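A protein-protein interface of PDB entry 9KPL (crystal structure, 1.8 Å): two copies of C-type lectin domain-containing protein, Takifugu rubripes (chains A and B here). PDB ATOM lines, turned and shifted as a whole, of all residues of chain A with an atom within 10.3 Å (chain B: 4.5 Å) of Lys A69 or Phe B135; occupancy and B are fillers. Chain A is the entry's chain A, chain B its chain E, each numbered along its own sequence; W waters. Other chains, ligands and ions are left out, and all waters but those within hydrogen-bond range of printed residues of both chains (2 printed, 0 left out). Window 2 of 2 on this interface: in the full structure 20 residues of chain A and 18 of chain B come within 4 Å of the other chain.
Printed residues of chain B within 4 Å of Lys A69: Ile B32, Ser B33, Ser B34, Met B70 and Phe B135. Of chain A, only Lys A69 comes within 4 Å of Phe B135. Of the printed residues of chain A, Ile B32 touches Asn A67 and Lys A69. Of the printed residues of chain B, Asn A67 touches Ile B32 (2.8 Å), Ser B33 (3.6 Å) and Ser B34 (3.9 Å). Of the printed residues of chain A, Met B70 touches Phe A68 and Lys A69. Of the printed residues of chain B, Phe A68 touches Met B70. The nearest residue of chain A that does not touch Phe B135 is Lys A123 (6.6 Å).
Among the printed residues, pairs that only touch across the chains: Phe A68 with Met B70 (3.1 Å), Lys A69 with Phe B135 (3.5 Å), Asn A67 with Ser B33 (3.6 Å), Lys A69 with Met B70 (3.8 Å), Lys A69 with Ser B34 (3.9 Å), Asn A67 with Ser B34 (3.9 Å) and Lys A69 with Ile B32 (3.96 Å).
Water W1 lies within hydrogen-bond range of the backbone carbonyl oxygen (O) of Ile B32 (2.8 Å), the side-chain amide oxygen (OD1) of Asn A67 (3.1 Å) and the backbone NH (N) of Ser B34 (3.3 Å). Water W2 lies within hydrogen-bond range of N of Ile B32 and ND2 of Asn A67.
Of the 23 printed residues of chain A, 3 touch a printed residue of chain B. Printed residues of chain B that touch a printed residue of chain A: Ile B32, Ser B33, Ser B34, Met B70 and Phe B135. Among the printed residues, 9 pairs touch across the chains.
O of Ile B32 lies within hydrogen-bond range of ND2 of Asn A67 (2.8 Å). The side-chain amino group of Lys A69 is in hydrogen-bond range of the backbone carbonyl oxygen of Ser B33, at 2.8 Å.
The backbone carbonyl oxygen of Asn A67 is in hydrogen-bond range of the side-chain amino group of Lys A69 (2.9 Å). O of Val B35 sits at hydrogen-bond distance from OG of Ser B33 (2.7 Å). The backbone carbonyl oxygen (O) of Tyr B136 lies within hydrogen-bond range of the backbone NH (N) of Ser B33 (2.9 Å). O of Phe B135 lies within hydrogen-bond range of N of Trp B73 (2.9 Å).
Positions printed for both chains: 32, 36, 70, 71, 72 and 135. Of the 9 pairs that touch across the chains among the printed residues, none has its exchanged pair printed and touching as well.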
ATOM      1  N   ILE A  32       8.082  23.412  23.743  1.00  0.00           N
ATOM      2  CA  ILE A  32       7.101  22.360  24.037  1.00  0.00           C
ATOM      3  C   ILE A  32       7.519  21.122  23.256  1.00  0.00           C
ATOM      4  O   ILE A  32       7.751  21.217  22.036  1.00  0.00           O
ATOM      5  CB  ILE A  32       5.675  22.813  23.645  1.00  0.00           C
ATOM      6  CG1 ILE A  32       5.253  23.963  24.570  1.00  0.00           C
ATOM      7  CG2 ILE A  32       4.648  21.629  23.711  1.00  0.00           C
ATOM      8  CD1 ILE A  32       3.908  24.637  24.188  1.00  0.00           C
ATOM      9  N   LYS A  36       5.900  12.525  24.381  1.00  0.00           N
ATOM     10  CA  LYS A  36       5.728  12.423  25.827  1.00  0.00           C
ATOM     11  C   LYS A  36       6.918  11.707  26.414  1.00  0.00           C
ATOM     12  O   LYS A  36       7.574  10.918  25.728  1.00  0.00           O
ATOM     13  CB  LYS A  36       4.441  11.639  26.132  1.00  0.00           C
ATOM     14  CG  LYS A  36       3.162  12.314  25.505  1.00  0.00           C
ATOM     15  CD  LYS A  36       1.882  11.747  26.099  1.00  0.00           C
ATOM     16  CE  LYS A  36       0.635  12.573  25.679  1.00  0.00           C
ATOM     17  NZ  LYS A  36      -0.577  11.973  26.358  1.00  0.00           N
ATOM     18  N   GLN A  62       2.062  31.442  34.983  1.00  0.00           N
ATOM     19  CA  GLN A  62       1.080  30.367  35.152  1.00  0.00           C
ATOM     20  C   GLN A  62      -0.042  30.475  34.117  1.00  0.00           C
ATOM     21  O   GLN A  62      -0.487  29.465  33.555  1.00  0.00           O
ATOM     22  CB  GLN A  62       0.494  30.373  36.573  1.00  0.00           C
ATOM     23  CG  GLN A  62      -0.580  29.308  36.746  1.00  0.00           C
ATOM     24  CD  GLN A  62      -0.078  27.870  36.597  1.00  0.00           C
ATOM     25  OE1 GLN A  62       1.114  27.588  36.778  1.00  0.00           O
ATOM     26  NE2 GLN A  62      -1.008  26.935  36.357  1.00  0.00           N
ATOM     27  N   ALA A  63      -0.555  31.691  33.878  1.00  0.00           N
ATOM     28  CA  ALA A  63      -1.635  31.828  32.905  1.00  0.00           C
ATOM     29  C   ALA A  63      -1.166  31.429  31.526  1.00  0.00           C
ATOM     30  O   ALA A  63      -1.904  30.761  30.780  1.00  0.00           O
ATOM     31  CB  ALA A  63      -2.140  33.281  32.851  1.00  0.00           C
ATOM     32  N   PHE A  64       0.049  31.863  31.170  1.00  0.00           N
ATOM     33  CA  PHE A  64       0.685  31.503  29.903  1.00  0.00           C
ATOM     34  C   PHE A  64       0.778  29.987  29.766  1.00  0.00           C
ATOM     35  O   PHE A  64       0.418  29.420  28.726  1.00  0.00           O
ATOM     36  CB  PHE A  64       2.059  32.215  29.881  1.00  0.00           C
ATOM     37  CG  PHE A  64       3.067  31.680  28.886  1.00  0.00           C
ATOM     38  CD1 PHE A  64       2.992  32.056  27.524  1.00  0.00           C
ATOM     39  CD2 PHE A  64       4.153  30.890  29.336  1.00  0.00           C
ATOM     40  CE1 PHE A  64       3.963  31.646  26.610  1.00  0.00           C
ATOM     41  CE2 PHE A  64       5.115  30.410  28.458  1.00  0.00           C
ATOM     42  CZ  PHE A  64       5.018  30.796  27.049  1.00  0.00           C
ATOM     43  N   LEU A  65       1.204  29.316  30.835  1.00  0.00           N
ATOM     44  CA  LEU A  65       1.302  27.855  30.862  1.00  0.00           C
ATOM     45  C   LEU A  65      -0.052  27.194  30.640  1.00  0.00           C
ATOM     46  O   LEU A  65      -0.192  26.249  29.828  1.00  0.00           O
ATOM     47  CB  LEU A  65       1.869  27.434  32.224  1.00  0.00           C
ATOM     48  CG  LEU A  65       1.824  25.924  32.554  1.00  0.00           C
ATOM     49  CD1 LEU A  65       2.741  25.132  31.590  1.00  0.00           C
ATOM     50  CD2 LEU A  65       2.241  25.625  34.063  1.00  0.00           C
ATOM     51  N   GLU A  66      -1.076  27.698  31.343  1.00  0.00           N
ATOM     52  CA  GLU A  66      -2.412  27.077  31.353  1.00  0.00           C
ATOM     53  C   GLU A  66      -3.079  27.189  29.982  1.00  0.00           C
ATOM     54  O   GLU A  66      -3.828  26.294  29.576  1.00  0.00           O
ATOM     55  CB  GLU A  66      -3.335  27.800  32.341  1.00  0.00           C
ATOM     56  CG  GLU A  66      -3.007  27.514  33.787  1.00  0.00           C
ATOM     57  CD  GLU A  66      -4.237  27.387  34.681  1.00  0.00           C
ATOM     58  OE1 GLU A  66      -5.332  27.909  34.328  1.00  0.00           O
ATOM     59  OE2 GLU A  66      -4.058  26.842  35.791  1.00  0.00           O
ATOM     60  N   ASN A  67      -2.793  28.270  29.270  1.00  0.00           N
ATOM     61  CA  ASN A  67      -3.512  28.573  28.035  1.00  0.00           C
ATOM     62  C   ASN A  67      -3.077  27.655  26.879  1.00  0.00           C
ATOM     63  O   ASN A  67      -3.722  27.673  25.814  1.00  0.00           O
ATOM     64  CB  ASN A  67      -3.270  30.042  27.694  1.00  0.00           C
ATOM     65  CG  ASN A  67      -4.209  30.561  26.601  1.00  0.00           C
ATOM     66  OD1 ASN A  67      -5.450  30.270  26.581  1.00  0.00           O
ATOM     67  ND2 ASN A  67      -3.607  31.223  25.620  1.00  0.00           N
ATOM     68  N   PHE A  68      -1.994  26.841  27.052  1.00  0.00           N
ATOM     69  CA  PHE A  68      -1.619  25.871  26.022  1.00  0.00           C
ATOM     70  C   PHE A  68      -2.556  24.680  26.024  1.00  0.00           C
ATOM     71  O   PHE A  68      -2.501  23.890  25.067  1.00  0.00           O
ATOM     72  CB  PHE A  68      -0.149  25.395  26.150  1.00  0.00           C
ATOM     73  CG  PHE A  68       0.803  26.511  25.825  1.00  0.00           C
ATOM     74  CD1 PHE A  68       0.731  27.110  24.556  1.00  0.00           C
ATOM     75  CD2 PHE A  68       1.621  27.052  26.786  1.00  0.00           C
ATOM     76  CE1 PHE A  68       1.496  28.292  24.237  1.00  0.00           C
ATOM     77  CE2 PHE A  68       2.428  28.144  26.468  1.00  0.00           C
ATOM     78  CZ  PHE A  68       2.354  28.760  25.186  1.00  0.00           C
ATOM     79  N   LYS A  69      -3.406  24.563  27.053  1.00  0.00           N
ATOM     80  CA  LYS A  69      -4.492  23.564  27.067  1.00  0.00           C
ATOM     81  C   LYS A  69      -3.896  22.185  26.800  1.00  0.00           C
ATOM     82  O   LYS A  69      -4.326  21.420  25.921  1.00  0.00           O
ATOM     83  CB  LYS A  69      -5.586  23.921  26.035  1.00  0.00           C
ATOM     84  CG  LYS A  69      -6.432  25.152  26.438  1.00  0.00           C
ATOM     85  CD  LYS A  69      -7.414  25.526  25.331  1.00  0.00           C
ATOM     86  CE  LYS A  69      -6.836  26.590  24.412  1.00  0.00           C
ATOM     87  NZ  LYS A  69      -6.603  27.810  25.276  1.00  0.00           N
ATOM     88  N   MET A  70      -2.824  21.905  27.528  1.00  0.00           N
ATOM     89  CA  MET A  70      -1.947  20.780  27.258  1.00  0.00           C
ATOM     90  C   MET A  70      -1.449  20.247  28.590  1.00  0.00           C
ATOM     91  O   MET A  70      -0.969  21.017  29.410  1.00  0.00           O
ATOM     92  CB  MET A  70      -0.689  21.206  26.473  1.00  0.00           C
ATOM     93  CG  MET A  70      -0.009  20.027  25.859  1.00  0.00           C
ATOM     94  SD  MET A  70       1.472  20.566  24.951  1.00  0.00           S
ATOM     95  CE  MET A  70       0.685  21.688  23.788  1.00  0.00           C
ATOM     96  N   THR A  71      -1.522  18.943  28.805  1.00  0.00           N
ATOM     97  CA  THR A  71      -0.943  18.427  30.062  1.00  0.00           C
ATOM     98  C   THR A  71       0.577  18.430  29.901  1.00  0.00           C
ATOM     99  O   THR A  71       1.111  17.872  28.927  1.00  0.00           O
ATOM    100  CB  THR A  71      -1.497  17.046  30.348  1.00  0.00           C
ATOM    101  OG1 THR A  71      -2.920  17.167  30.494  1.00  0.00           O
ATOM    102  CG2 THR A  71      -0.904  16.461  31.645  1.00  0.00           C
ATOM    103  N   LEU A  72       1.268  19.112  30.812  1.00  0.00           N
ATOM    104  CA  LEU A  72       2.699  19.329  30.684  1.00  0.00           C
ATOM    105  C   LEU A  72       3.414  18.994  31.996  1.00  0.00           C
ATOM    106  O   LEU A  72       3.009  19.499  33.044  1.00  0.00           O
ATOM    107  CB  LEU A  72       2.985  20.808  30.359  1.00  0.00           C
ATOM    108  CG  LEU A  72       2.590  21.124  28.933  1.00  0.00           C
ATOM    109  CD1 LEU A  72       2.539  22.650  28.758  1.00  0.00           C
ATOM    110  CD2 LEU A  72       3.645  20.454  27.971  1.00  0.00           C
ATOM    111  N   GLN A 116       1.190  20.178  34.942  1.00  0.00           N
ATOM    112  CA  GLN A 116       0.057  21.065  34.699  1.00  0.00           C
ATOM    113  C   GLN A 116      -1.001  20.241  33.974  1.00  0.00           C
ATOM    114  O   GLN A 116      -0.725  19.647  32.933  1.00  0.00           O
ATOM    115  CB  GLN A 116       0.490  22.254  33.830  1.00  0.00           C
ATOM    116  CG  GLN A 116      -0.667  23.154  33.236  1.00  0.00           C
ATOM    117  CD  GLN A 116      -1.381  23.930  34.323  1.00  0.00           C
ATOM    118  OE1 GLN A 116      -0.827  24.160  35.404  1.00  0.00           O
ATOM    119  NE2 GLN A 116      -2.629  24.291  34.073  1.00  0.00           N
ATOM    120  N   ILE A 117      -2.202  20.221  34.498  1.00  0.00           N
ATOM    121  CA  ILE A 117      -3.241  19.378  33.911  1.00  0.00           C
ATOM    122  C   ILE A 117      -4.062  20.193  32.942  1.00  0.00           C
ATOM    123  O   ILE A 117      -4.104  21.431  32.989  1.00  0.00           O
ATOM    124  CB  ILE A 117      -4.128  18.728  34.968  1.00  0.00           C
ATOM    125  CG1 ILE A 117      -5.098  19.772  35.506  1.00  0.00           C
ATOM    126  CG2 ILE A 117      -3.304  18.094  36.025  1.00  0.00           C
ATOM    127  CD1 ILE A 117      -5.775  19.329  36.784  1.00  0.00           C
ATOM    128  N   ASP A 118      -4.730  19.478  32.049  1.00  0.00           N
ATOM    129  CA  ASP A 118      -5.652  20.058  31.074  1.00  0.00           C
ATOM    130  C   ASP A 118      -6.961  19.288  31.202  1.00  0.00           C
ATOM    131  O   ASP A 118      -7.129  18.249  30.559  1.00  0.00           O
ATOM    132  CB  ASP A 118      -5.044  19.951  29.662  1.00  0.00           C
ATOM    133  CG  ASP A 118      -6.084  20.103  28.556  1.00  0.00           C
ATOM    134  OD1 ASP A 118      -6.741  21.159  28.578  1.00  0.00           O
ATOM    135  OD2 ASP A 118      -6.189  19.195  27.662  1.00  0.00           O
ATOM    136  N   ARG A 119      -7.855  19.734  32.077  1.00  0.00           N
ATOM    137  CA  ARG A 119      -9.070  18.965  32.320  1.00  0.00           C
ATOM    138  C   ARG A 119     -10.266  19.898  32.361  1.00  0.00           C
ATOM    139  O   ARG A 119     -10.148  21.082  32.696  1.00  0.00           O
ATOM    140  CB  ARG A 119      -9.005  18.147  33.626  1.00  0.00           C
ATOM    141  CG  ARG A 119      -8.034  16.973  33.586  1.00  0.00           C
ATOM    142  CD  ARG A 119      -7.974  16.284  34.943  1.00  0.00           C
ATOM    143  NE  ARG A 119      -9.232  15.649  35.324  1.00  0.00           N
ATOM    144  CZ  ARG A 119      -9.485  14.352  35.189  1.00  0.00           C
ATOM    145  NH1 ARG A 119      -8.561  13.509  34.746  1.00  0.00           N
ATOM    146  NH2 ARG A 119     -10.697  13.890  35.505  1.00  0.00           N
ATOM    147  N   GLU A 120     -11.419  19.348  31.989  1.00  0.00           N
ATOM    148  CA  GLU A 120     -12.663  20.085  32.120  1.00  0.00           C
ATOM    149  C   GLU A 120     -12.964  20.268  33.603  1.00  0.00           C
ATOM    150  O   GLU A 120     -13.006  19.289  34.362  1.00  0.00           O
ATOM    151  CB  GLU A 120     -13.796  19.326  31.427  1.00  0.00           C
ATOM    152  CG  GLU A 120     -13.667  19.152  29.901  1.00  0.00           C
ATOM    153  CD  GLU A 120     -13.588  20.464  29.119  1.00  0.00           C
ATOM    154  OE1 GLU A 120     -14.321  21.422  29.469  1.00  0.00           O
ATOM    155  OE2 GLU A 120     -12.812  20.524  28.135  1.00  0.00           O
ATOM    156  N   LYS A 122     -11.133  21.376  35.954  1.00  0.00           N
ATOM    157  CA  LYS A 122     -10.008  21.162  36.872  1.00  0.00           C
ATOM    158  C   LYS A 122      -8.741  21.582  36.126  1.00  0.00           C
ATOM    159  O   LYS A 122      -8.257  20.826  35.278  1.00  0.00           O
ATOM    160  CB  LYS A 122      -9.917  19.708  37.323  1.00  0.00           C
ATOM    161  CG  LYS A 122      -9.368  19.541  38.728  1.00  0.00           C
ATOM    162  CD  LYS A 122      -9.071  18.081  39.089  1.00  0.00           C
ATOM    163  CE  LYS A 122      -7.901  17.981  40.104  1.00  0.00           C
ATOM    164  NZ  LYS A 122      -6.768  17.052  39.649  1.00  0.00           N
ATOM    165  N   LYS A 123      -8.215  22.768  36.440  1.00  0.00           N
ATOM    166  CA  LYS A 123      -6.947  23.199  35.857  1.00  0.00           C
ATOM    167  C   LYS A 123      -5.988  23.628  36.965  1.00  0.00           C
ATOM    168  O   LYS A 123      -6.405  23.909  38.090  1.00  0.00           O
ATOM    169  CB  LYS A 123      -7.161  24.310  34.808  1.00  0.00           C
ATOM    170  CG  LYS A 123      -7.993  23.745  33.644  1.00  0.00           C
ATOM    171  CD  LYS A 123      -8.203  24.652  32.420  1.00  0.00           C
ATOM    172  CE  LYS A 123      -9.098  23.887  31.399  1.00  0.00           C
ATOM    173  NZ  LYS A 123      -9.353  24.600  30.120  1.00  0.00           N
ATOM    174  N   GLY A 124      -4.686  23.628  36.652  1.00  0.00           N
ATOM    175  CA  GLY A 124      -3.658  23.876  37.650  1.00  0.00           C
ATOM    176  C   GLY A 124      -2.816  22.632  37.827  1.00  0.00           C
ATOM    177  O   GLY A 124      -2.903  21.663  37.058  1.00  0.00           O
ATOM    178  N   PHE A 135       3.753  15.167  27.639  1.00  0.00           N
ATOM    179  CA  PHE A 135       4.492  16.232  26.997  1.00  0.00           C
ATOM    180  C   PHE A 135       5.138  17.092  28.080  1.00  0.00           C
ATOM    181  O   PHE A 135       4.728  17.063  29.245  1.00  0.00           O
ATOM    182  CB  PHE A 135       3.536  17.114  26.170  1.00  0.00           C
ATOM    183  CG  PHE A 135       2.916  16.356  25.005  1.00  0.00           C
ATOM    184  CD1 PHE A 135       3.757  15.783  24.059  1.00  0.00           C
ATOM    185  CD2 PHE A 135       1.541  16.240  24.883  1.00  0.00           C
ATOM    186  CE1 PHE A 135       3.252  15.078  22.950  1.00  0.00           C
ATOM    187  CE2 PHE A 135       0.984  15.467  23.806  1.00  0.00           C
ATOM    188  CZ  PHE A 135       1.880  14.911  22.827  1.00  0.00           C
ATOM    189  N   MET A 137       7.581  20.959  28.932  1.00  0.00           N
ATOM    190  CA  MET A 137       7.938  22.317  28.526  1.00  0.00           C
ATOM    191  C   MET A 137       9.294  22.651  29.149  1.00  0.00           C
ATOM    192  O   MET A 137       9.431  22.543  30.388  1.00  0.00           O
ATOM    193  CB  MET A 137       6.886  23.330  29.017  1.00  0.00           C
ATOM    194  CG  MET A 137       7.319  24.865  28.740  1.00  0.00           C
ATOM    195  SD  MET A 137       6.053  25.938  29.373  1.00  0.00           S
ATOM    196  CE  MET A 137       5.045  26.013  27.865  1.00  0.00           C
ATOM    197  N   ILE B  32      -3.351  32.667  21.610  1.00  0.00           N
ATOM    198  CA  ILE B  32      -4.213  31.487  21.484  1.00  0.00           C
ATOM    199  C   ILE B  32      -5.440  31.746  22.330  1.00  0.00           C
ATOM    200  O   ILE B  32      -5.290  32.092  23.512  1.00  0.00           O
ATOM    201  CB  ILE B  32      -3.472  30.221  21.957  1.00  0.00           C
ATOM    202  CG1 ILE B  32      -2.391  29.864  20.965  1.00  0.00           C
ATOM    203  CG2 ILE B  32      -4.439  29.023  22.187  1.00  0.00           C
ATOM    204  CD1 ILE B  32      -1.435  28.779  21.542  1.00  0.00           C
ATOM    205  N   SER B  33      -6.654  31.632  21.716  1.00  0.00           N
ATOM    206  CA  SER B  33      -7.901  31.931  22.437  1.00  0.00           C
ATOM    207  C   SER B  33      -8.130  30.987  23.624  1.00  0.00           C
ATOM    208  O   SER B  33      -7.630  29.852  23.691  1.00  0.00           O
ATOM    209  CB  SER B  33      -9.086  31.844  21.465  1.00  0.00           C
ATOM    210  OG  SER B  33      -9.267  30.474  21.157  1.00  0.00           O
ATOM    211  N   SER B  34      -8.933  31.462  24.591  1.00  0.00           N
ATOM    212  CA  SER B  34      -9.362  30.523  25.620  1.00  0.00           C
ATOM    213  C   SER B  34     -10.785  30.049  25.382  1.00  0.00           C
ATOM    214  O   SER B  34     -11.270  29.212  26.144  1.00  0.00           O
ATOM    215  CB  SER B  34      -9.232  31.143  27.016  1.00  0.00           C
ATOM    216  OG  SER B  34     -10.054  32.302  27.083  1.00  0.00           O
ATOM    217  N   VAL B  35     -11.402  30.459  24.261  1.00  0.00           N
ATOM    218  CA  VAL B  35     -12.723  29.962  23.899  1.00  0.00           C
ATOM    219  C   VAL B  35     -12.715  29.534  22.435  1.00  0.00           C
ATOM    220  O   VAL B  35     -11.847  29.936  21.655  1.00  0.00           O
ATOM    221  CB  VAL B  35     -13.807  31.032  24.138  1.00  0.00           C
ATOM    222  CG1 VAL B  35     -13.817  31.400  25.643  1.00  0.00           C
ATOM    223  CG2 VAL B  35     -13.574  32.245  23.221  1.00  0.00           C
ATOM    224  N   LYS B  36     -13.722  28.743  22.060  1.00  0.00           N
ATOM    225  CA  LYS B  36     -13.911  28.404  20.653  1.00  0.00           C
ATOM    226  C   LYS B  36     -14.863  29.412  20.041  1.00  0.00           C
ATOM    227  O   LYS B  36     -15.709  30.008  20.732  1.00  0.00           O
ATOM    228  CB  LYS B  36     -14.472  26.980  20.503  1.00  0.00           C
ATOM    229  CG  LYS B  36     -13.512  25.888  21.115  1.00  0.00           C
ATOM    230  CD  LYS B  36     -13.878  24.465  20.651  1.00  0.00           C
ATOM    231  CE  LYS B  36     -12.926  23.397  21.207  1.00  0.00           C
ATOM    232  NZ  LYS B  36     -13.187  22.045  20.577  1.00  0.00           N
ATOM    233  N   MET B  70      -3.035  21.515  18.704  1.00  0.00           N
ATOM    234  CA  MET B  70      -4.306  22.163  18.987  1.00  0.00           C
ATOM    235  C   MET B  70      -4.993  22.420  17.660  1.00  0.00           C
ATOM    236  O   MET B  70      -4.344  22.878  16.721  1.00  0.00           O
ATOM    237  CB  MET B  70      -4.082  23.510  19.711  1.00  0.00           C
ATOM    238  CG  MET B  70      -5.334  24.119  20.302  1.00  0.00           C
ATOM    239  SD  MET B  70      -4.879  25.630  21.139  1.00  0.00           S
ATOM    240  CE  MET B  70      -3.873  25.017  22.525  1.00  0.00           C
ATOM    241  N   THR B  71      -6.278  22.122  17.578  1.00  0.00           N
ATOM    242  CA  THR B  71      -7.013  22.520  16.371  1.00  0.00           C
ATOM    243  C   THR B  71      -7.303  24.013  16.482  1.00  0.00           C
ATOM    244  O   THR B  71      -7.926  24.462  17.467  1.00  0.00           O
ATOM    245  CB  THR B  71      -8.300  21.726  16.248  1.00  0.00           C
ATOM    246  OG1 THR B  71      -7.947  20.343  16.267  1.00  0.00           O
ATOM    247  CG2 THR B  71      -9.002  22.104  14.913  1.00  0.00           C
ATOM    248  N   LEU B  72      -6.814  24.781  15.505  1.00  0.00           N
ATOM    249  CA  LEU B  72      -6.881  26.236  15.511  1.00  0.00           C
ATOM    250  C   LEU B  72      -7.404  26.764  14.181  1.00  0.00           C
ATOM    251  O   LEU B  72      -6.926  26.338  13.136  1.00  0.00           O
ATOM    252  CB  LEU B  72      -5.467  26.841  15.708  1.00  0.00           C
ATOM    253  CG  LEU B  72      -4.949  26.584  17.106  1.00  0.00           C
ATOM    254  CD1 LEU B  72      -3.439  26.824  17.180  1.00  0.00           C
ATOM    255  CD2 LEU B  72      -5.710  27.588  18.068  1.00  0.00           C
ATOM    256  N   TRP B  73      -8.361  27.719  14.214  1.00  0.00           N
ATOM    257  CA  TRP B  73      -8.622  28.505  13.013  1.00  0.00           C
ATOM    258  C   TRP B  73      -7.371  29.314  12.677  1.00  0.00           C
ATOM    259  O   TRP B  73      -6.743  29.873  13.574  1.00  0.00           O
ATOM    260  CB  TRP B  73      -9.762  29.527  13.239  1.00  0.00           C
ATOM    261  CG  TRP B  73     -11.122  28.981  13.279  1.00  0.00           C
ATOM    262  CD1 TRP B  73     -12.083  29.241  14.247  1.00  0.00           C
ATOM    263  CD2 TRP B  73     -11.780  28.195  12.254  1.00  0.00           C
ATOM    264  NE1 TRP B  73     -13.264  28.610  13.903  1.00  0.00           N
ATOM    265  CE2 TRP B  73     -13.106  27.972  12.698  1.00  0.00           C
ATOM    266  CE3 TRP B  73     -11.344  27.583  11.049  1.00  0.00           C
ATOM    267  CZ2 TRP B  73     -14.020  27.216  11.966  1.00  0.00           C
ATOM    268  CZ3 TRP B  73     -12.296  26.816  10.293  1.00  0.00           C
ATOM    269  CH2 TRP B  73     -13.620  26.688  10.776  1.00  0.00           C
ATOM    270  N   ASN B 134     -13.871  26.600  16.723  1.00  0.00           N
ATOM    271  CA  ASN B 134     -12.542  26.103  17.079  1.00  0.00           C
ATOM    272  C   ASN B 134     -11.924  27.174  17.952  1.00  0.00           C
ATOM    273  O   ASN B 134     -12.298  28.337  17.824  1.00  0.00           O
ATOM    274  CB  ASN B 134     -11.578  25.969  15.852  1.00  0.00           C
ATOM    275  CG  ASN B 134     -11.823  24.733  15.050  1.00  0.00           C
ATOM    276  OD1 ASN B 134     -11.973  23.604  15.603  1.00  0.00           O
ATOM    277  ND2 ASN B 134     -11.820  24.902  13.725  1.00  0.00           N
ATOM    278  N   PHE B 135     -10.951  26.785  18.788  1.00  0.00           N
ATOM    279  CA  PHE B 135      -9.949  27.760  19.250  1.00  0.00           C
ATOM    280  C   PHE B 135      -9.294  28.422  18.044  1.00  0.00           C
ATOM    281  O   PHE B 135      -9.314  27.896  16.924  1.00  0.00           O
ATOM    282  CB  PHE B 135      -8.825  27.108  20.077  1.00  0.00           C
ATOM    283  CG  PHE B 135      -9.365  26.420  21.335  1.00  0.00           C
ATOM    284  CD1 PHE B 135     -10.013  27.177  22.321  1.00  0.00           C
ATOM    285  CD2 PHE B 135      -9.278  25.068  21.479  1.00  0.00           C
ATOM    286  CE1 PHE B 135     -10.591  26.569  23.479  1.00  0.00           C
ATOM    287  CE2 PHE B 135      -9.840  24.400  22.638  1.00  0.00           C
ATOM    288  CZ  PHE B 135     -10.500  25.182  23.623  1.00  0.00           C
ATOM    289  N   TYR B 136      -8.760  29.624  18.276  1.00  0.00           N
ATOM    290  CA  TYR B 136      -8.174  30.390  17.178  1.00  0.00           C
ATOM    291  C   TYR B 136      -6.882  31.061  17.635  1.00  0.00           C
ATOM    292  O   TYR B 136      -6.653  31.306  18.815  1.00  0.00           O
ATOM    293  CB  TYR B 136      -9.136  31.464  16.653  1.00  0.00           C
ATOM    294  CG  TYR B 136      -9.751  32.334  17.748  1.00  0.00           C
ATOM    295  CD1 TYR B 136     -10.904  31.918  18.426  1.00  0.00           C
ATOM    296  CD2 TYR B 136      -9.207  33.594  18.039  1.00  0.00           C
ATOM    297  CE1 TYR B 136     -11.506  32.750  19.393  1.00  0.00           C
ATOM    298  CE2 TYR B 136      -9.763  34.421  18.990  1.00  0.00           C
ATOM    299  CZ  TYR B 136     -10.892  33.993  19.664  1.00  0.00           C
ATOM    300  OH  TYR B 136     -11.452  34.812  20.597  1.00  0.00           O
HETATM  301  O   HOH W   1      -6.373  33.160  25.882  1.00  0.00           O
HETATM  302  O   HOH W   2      -2.431  33.484  24.230  1.00  0.00           O
